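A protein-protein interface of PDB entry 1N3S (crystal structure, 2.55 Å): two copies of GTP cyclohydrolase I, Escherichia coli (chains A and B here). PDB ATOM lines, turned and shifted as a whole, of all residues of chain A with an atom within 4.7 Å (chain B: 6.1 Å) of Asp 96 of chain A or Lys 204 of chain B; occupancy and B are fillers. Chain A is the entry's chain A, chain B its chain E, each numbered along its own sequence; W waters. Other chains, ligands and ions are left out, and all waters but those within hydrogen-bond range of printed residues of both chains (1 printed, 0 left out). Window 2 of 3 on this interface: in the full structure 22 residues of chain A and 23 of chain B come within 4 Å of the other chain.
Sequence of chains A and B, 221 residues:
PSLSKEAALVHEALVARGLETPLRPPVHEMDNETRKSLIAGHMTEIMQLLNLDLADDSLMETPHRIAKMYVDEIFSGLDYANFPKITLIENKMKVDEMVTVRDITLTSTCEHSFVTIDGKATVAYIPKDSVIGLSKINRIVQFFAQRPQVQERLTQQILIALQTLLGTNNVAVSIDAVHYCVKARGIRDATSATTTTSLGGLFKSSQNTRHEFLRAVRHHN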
ATOM      1  N   LYS A  94       1.629   5.957  34.434  1.00  0.00           N
ATOM      2  CA  LYS A  94       2.958   6.438  33.977  1.00  0.00           C
ATOM      3  C   LYS A  94       3.776   5.469  33.139  1.00  0.00           C
ATOM      4  O   LYS A  94       5.006   5.462  33.201  1.00  0.00           O
ATOM      5  CB  LYS A  94       3.786   6.943  35.160  1.00  0.00           C
ATOM      6  CG  LYS A  94       3.507   8.381  35.485  1.00  0.00           C
ATOM      7  CD  LYS A  94       3.675   8.647  36.960  1.00  0.00           C
ATOM      8  CE  LYS A  94       3.234  10.058  37.299  1.00  0.00           C
ATOM      9  NZ  LYS A  94       2.973  10.186  38.757  1.00  0.00           N
ATOM     10  N   VAL A  95       3.087   4.703  32.298  1.00  0.00           N
ATOM     11  CA  VAL A  95       3.783   3.713  31.508  1.00  0.00           C
ATOM     12  C   VAL A  95       4.501   4.140  30.244  1.00  0.00           C
ATOM     13  O   VAL A  95       3.962   4.790  29.340  1.00  0.00           O
ATOM     14  CB  VAL A  95       3.002   2.416  31.268  1.00  0.00           C
ATOM     15  CG1 VAL A  95       3.942   1.252  31.451  1.00  0.00           C
ATOM     16  CG2 VAL A  95       1.819   2.267  32.201  1.00  0.00           C
ATOM     17  N   ASP A  96       5.756   3.720  30.249  1.00  0.00           N
ATOM     18  CA  ASP A  96       6.748   3.896  29.213  1.00  0.00           C
ATOM     19  C   ASP A  96       6.688   2.674  28.241  1.00  0.00           C
ATOM     20  O   ASP A  96       7.678   2.341  27.562  1.00  0.00           O
ATOM     21  CB  ASP A  96       8.109   3.996  29.916  1.00  0.00           C
ATOM     22  CG  ASP A  96       8.286   2.940  31.028  1.00  0.00           C
ATOM     23  OD1 ASP A  96       8.191   3.298  32.221  1.00  0.00           O
ATOM     24  OD2 ASP A  96       8.518   1.749  30.714  1.00  0.00           O
ATOM     25  N   GLU A  97       5.513   2.028  28.210  1.00  0.00           N
ATOM     26  CA  GLU A  97       5.214   0.849  27.382  1.00  0.00           C
ATOM     27  C   GLU A  97       4.753   1.147  25.943  1.00  0.00           C
ATOM     28  O   GLU A  97       4.327   2.250  25.635  1.00  0.00           O
ATOM     29  CB  GLU A  97       4.202  -0.058  28.123  1.00  0.00           C
ATOM     30  CG  GLU A  97       2.875  -0.387  27.411  1.00  0.00           C
ATOM     31  CD  GLU A  97       1.754  -0.806  28.327  1.00  0.00           C
ATOM     32  OE1 GLU A  97       1.837  -0.624  29.560  1.00  0.00           O
ATOM     33  OE2 GLU A  97       0.748  -1.308  27.792  1.00  0.00           O
ATOM     34  N   MET A  98       4.815   0.134  25.080  1.00  0.00           N
ATOM     35  CA  MET A  98       4.404   0.268  23.680  1.00  0.00           C
ATOM     36  C   MET A  98       3.076  -0.423  23.302  1.00  0.00           C
ATOM     37  O   MET A  98       2.785  -1.542  23.741  1.00  0.00           O
ATOM     38  CB  MET A  98       5.574  -0.127  22.761  1.00  0.00           C
ATOM     39  CG  MET A  98       5.253  -0.942  21.526  1.00  0.00           C
ATOM     40  SD  MET A  98       6.527  -0.711  20.334  1.00  0.00           S
ATOM     41  CE  MET A  98       5.628  -0.593  18.985  1.00  0.00           C
ATOM     42  N   ILE A 126       4.115   5.079  21.756  1.00  0.00           N
ATOM     43  CA  ILE A 126       4.569   4.957  23.134  1.00  0.00           C
ATOM     44  C   ILE A 126       3.876   6.091  23.915  1.00  0.00           C
ATOM     45  O   ILE A 126       4.147   7.268  23.669  1.00  0.00           O
ATOM     46  CB  ILE A 126       6.133   5.014  23.245  1.00  0.00           C
ATOM     47  CG1 ILE A 126       6.734   3.775  22.561  1.00  0.00           C
ATOM     48  CG2 ILE A 126       6.579   5.047  24.726  1.00  0.00           C
ATOM     49  CD1 ILE A 126       8.219   3.798  22.354  1.00  0.00           C
ATOM     50  N   THR B 197       2.731  -4.181  24.955  1.00  0.00           N
ATOM     51  CA  THR B 197       3.951  -4.761  25.535  1.00  0.00           C
ATOM     52  C   THR B 197       4.622  -3.907  26.627  1.00  0.00           C
ATOM     53  O   THR B 197       4.993  -2.765  26.381  1.00  0.00           O
ATOM     54  CB  THR B 197       5.049  -5.158  24.437  1.00  0.00           C
ATOM     55  OG1 THR B 197       5.946  -4.069  24.201  1.00  0.00           O
ATOM     56  CG2 THR B 197       4.431  -5.537  23.098  1.00  0.00           C
ATOM     57  N   LEU B 199       7.883  -3.806  28.895  1.00  0.00           N
ATOM     58  CA  LEU B 199       9.243  -4.315  29.069  1.00  0.00           C
ATOM     59  C   LEU B 199       9.870  -3.817  30.362  1.00  0.00           C
ATOM     60  O   LEU B 199       9.725  -2.639  30.710  1.00  0.00           O
ATOM     61  CB  LEU B 199      10.118  -3.886  27.882  1.00  0.00           C
ATOM     62  CG  LEU B 199       9.538  -3.966  26.463  1.00  0.00           C
ATOM     63  CD1 LEU B 199      10.521  -3.402  25.459  1.00  0.00           C
ATOM     64  CD2 LEU B 199       9.161  -5.394  26.110  1.00  0.00           C
ATOM     65  N   GLY B 200      10.577  -4.707  31.055  1.00  0.00           N
ATOM     66  CA  GLY B 200      11.241  -4.342  32.295  1.00  0.00           C
ATOM     67  C   GLY B 200      12.678  -4.824  32.350  1.00  0.00           C
ATOM     68  O   GLY B 200      13.037  -5.786  31.667  1.00  0.00           O
ATOM     69  N   GLY B 201      13.496  -4.149  33.164  1.00  0.00           N
ATOM     70  CA  GLY B 201      14.903  -4.502  33.346  1.00  0.00           C
ATOM     71  C   GLY B 201      15.756  -4.582  32.096  1.00  0.00           C
ATOM     72  O   GLY B 201      15.787  -3.630  31.315  1.00  0.00           O
ATOM     73  N   LEU B 202      16.404  -5.735  31.893  1.00  0.00           N
ATOM     74  CA  LEU B 202      17.265  -5.979  30.731  1.00  0.00           C
ATOM     75  C   LEU B 202      16.462  -6.040  29.426  1.00  0.00           C
ATOM     76  O   LEU B 202      17.003  -5.797  28.345  1.00  0.00           O
ATOM     77  CB  LEU B 202      18.120  -7.246  30.923  1.00  0.00           C
ATOM     78  CG  LEU B 202      19.241  -7.285  31.991  1.00  0.00           C
ATOM     79  CD1 LEU B 202      19.664  -8.733  32.286  1.00  0.00           C
ATOM     80  CD2 LEU B 202      20.451  -6.440  31.602  1.00  0.00           C
ATOM     81  N   PHE B 203      15.159  -6.311  29.543  1.00  0.00           N
ATOM     82  CA  PHE B 203      14.254  -6.352  28.391  1.00  0.00           C
ATOM     83  C   PHE B 203      13.920  -4.923  27.954  1.00  0.00           C
ATOM     84  O   PHE B 203      13.364  -4.714  26.877  1.00  0.00           O
ATOM     85  CB  PHE B 203      12.953  -7.098  28.722  1.00  0.00           C
ATOM     86  CG  PHE B 203      13.123  -8.572  28.920  1.00  0.00           C
ATOM     87  CD1 PHE B 203      13.227  -9.434  27.820  1.00  0.00           C
ATOM     88  CD2 PHE B 203      13.130  -9.120  30.207  1.00  0.00           C
ATOM     89  CE1 PHE B 203      13.334 -10.846  27.994  1.00  0.00           C
ATOM     90  CE2 PHE B 203      13.237 -10.531  30.409  1.00  0.00           C
ATOM     91  CZ  PHE B 203      13.338 -11.393  29.298  1.00  0.00           C
ATOM     92  N   LYS B 204      14.265  -3.957  28.807  1.00  0.00           N
ATOM     93  CA  LYS B 204      14.030  -2.539  28.551  1.00  0.00           C
ATOM     94  C   LYS B 204      15.346  -1.779  28.349  1.00  0.00           C
ATOM     95  O   LYS B 204      15.664  -1.389  27.227  1.00  0.00           O
ATOM     96  CB  LYS B 204      13.230  -1.917  29.703  1.00  0.00           C
ATOM     97  CG  LYS B 204      12.733  -0.502  29.442  1.00  0.00           C
ATOM     98  CD  LYS B 204      12.119   0.113  30.686  1.00  0.00           C
ATOM     99  CE  LYS B 204      11.870   1.595  30.476  1.00  0.00           C
ATOM    100  NZ  LYS B 204      10.964   1.852  29.316  1.00  0.00           N
ATOM    101  N   SER B 205      16.100  -1.583  29.439  1.00  0.00           N
ATOM    102  CA  SER B 205      17.385  -0.859  29.438  1.00  0.00           C
ATOM    103  C   SER B 205      18.434  -1.418  28.472  1.00  0.00           C
ATOM    104  O   SER B 205      18.868  -0.709  27.557  1.00  0.00           O
ATOM    105  CB  SER B 205      17.954  -0.761  30.865  1.00  0.00           C
ATOM    106  OG  SER B 205      18.073  -2.033  31.487  1.00  0.00           O
ATOM    107  N   SER B 206      18.801  -2.690  28.654  1.00  0.00           N
ATOM    108  CA  SER B 206      19.775  -3.359  27.785  1.00  0.00           C
ATOM    109  C   SER B 206      19.192  -3.593  26.390  1.00  0.00           C
ATOM    110  O   SER B 206      18.079  -4.113  26.240  1.00  0.00           O
ATOM    111  CB  SER B 206      20.256  -4.686  28.391  1.00  0.00           C
ATOM    112  OG  SER B 206      21.102  -5.423  27.510  1.00  0.00           O
ATOM    113  N   GLN B 207      19.982  -3.197  25.396  1.00  0.00           N
ATOM    114  CA  GLN B 207      19.667  -3.280  23.970  1.00  0.00           C
ATOM    115  C   GLN B 207      19.498  -4.710  23.437  1.00  0.00           C
ATOM    116  O   GLN B 207      18.632  -4.975  22.599  1.00  0.00           O
ATOM    117  CB  GLN B 207      20.785  -2.557  23.197  1.00  0.00           C
ATOM    118  CG  GLN B 207      20.524  -2.273  21.721  1.00  0.00           C
ATOM    119  CD  GLN B 207      19.273  -1.460  21.498  1.00  0.00           C
ATOM    120  OE1 GLN B 207      19.098  -0.381  22.077  1.00  0.00           O
ATOM    121  NE2 GLN B 207      18.378  -1.986  20.671  1.00  0.00           N
ATOM    122  N   THR B 209      18.818  -7.925  25.230  1.00  0.00           N
ATOM    123  CA  THR B 209      17.677  -8.693  25.736  1.00  0.00           C
ATOM    124  C   THR B 209      16.317  -8.112  25.343  1.00  0.00           C
ATOM    125  O   THR B 209      15.294  -8.809  25.404  1.00  0.00           O
ATOM    126  CB  THR B 209      17.793  -8.936  27.267  1.00  0.00           C
ATOM    127  OG1 THR B 209      19.160  -9.192  27.605  1.00  0.00           O
ATOM    128  CG2 THR B 209      16.992 -10.153  27.695  1.00  0.00           C
ATOM    129  N   ARG B 210      16.344  -6.878  24.832  1.00  0.00           N
ATOM    130  CA  ARG B 210      15.155  -6.158  24.377  1.00  0.00           C
ATOM    131  C   ARG B 210      14.598  -6.819  23.122  1.00  0.00           C
ATOM    132  O   ARG B 210      13.424  -7.170  23.083  1.00  0.00           O
ATOM    133  CB  ARG B 210      15.504  -4.680  24.129  1.00  0.00           C
ATOM    134  CG  ARG B 210      14.323  -3.732  23.939  1.00  0.00           C
ATOM    135  CD  ARG B 210      14.717  -2.304  24.277  1.00  0.00           C
ATOM    136  NE  ARG B 210      13.664  -1.344  23.940  1.00  0.00           N
ATOM    137  CZ  ARG B 210      13.149  -0.435  24.770  1.00  0.00           C
ATOM    138  NH1 ARG B 210      13.575  -0.330  26.021  1.00  0.00           N
ATOM    139  NH2 ARG B 210      12.204   0.392  24.339  1.00  0.00           N
HETATM  140  O   HOH W   1       9.205   0.113  25.974  1.00  0.00           O
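O of Met 98 of chain A lies within hydrogen-bond range of N of Thr 197 of chain B, 2.9 Å away.
The side-chain carboxylate (OD2) of Asp 96 of chain A is in salt-bridge range of the side-chain amino group (NZ) of Lys 204 of chain B.
The backbone carbonyl oxygen (O) of Lys 204 of chain B is in hydrogen-bond range of the guanidinium group (NH1) of Arg 210 of chain B (2.6 Å).
Among the printed residues, merely in contact across the chains: Glu 97 of chain A with Thr 197 of chain B.
Lys 204 of chain B touches one residue of chain A.
Of the printed residues of chain B, Met 98 of chain A touches Thr 197.
Printed residues of chain A within 4 Å of Thr 197 of chain B: Glu 97 and Met 98.
Printed residues of chain B within 4 Å of Glu 97 of chain A: Thr 197.
Phe 203 of chain B touches none of the printed residues of chain A.
Gly 201 of chain B touches none of the printed residues of chain A.
The nearest printed residue of chain A that does not touch Lys 204 of chain B is Glu 97 of chain A (5.6 Å).
Along chain B the printed residues that touch a printed residue of chain A span positions 197 to 204.
Among the printed residues, 3 pairs touch across the chains.
Among the printed residues, Asp or Glu carboxylates within 4 Å of a Lys or Arg side-chain nitrogen of the other chain: Asp 96 of chain A with Lys 204 of chain B (2.8 Å).
No position is printed for both chains.
Water W1 bridges the backbone carbonyl oxygen of Asp 96 of chain A (3.1 Å) and the guanidinium group of Arg 210 of chain B (3.4 Å).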
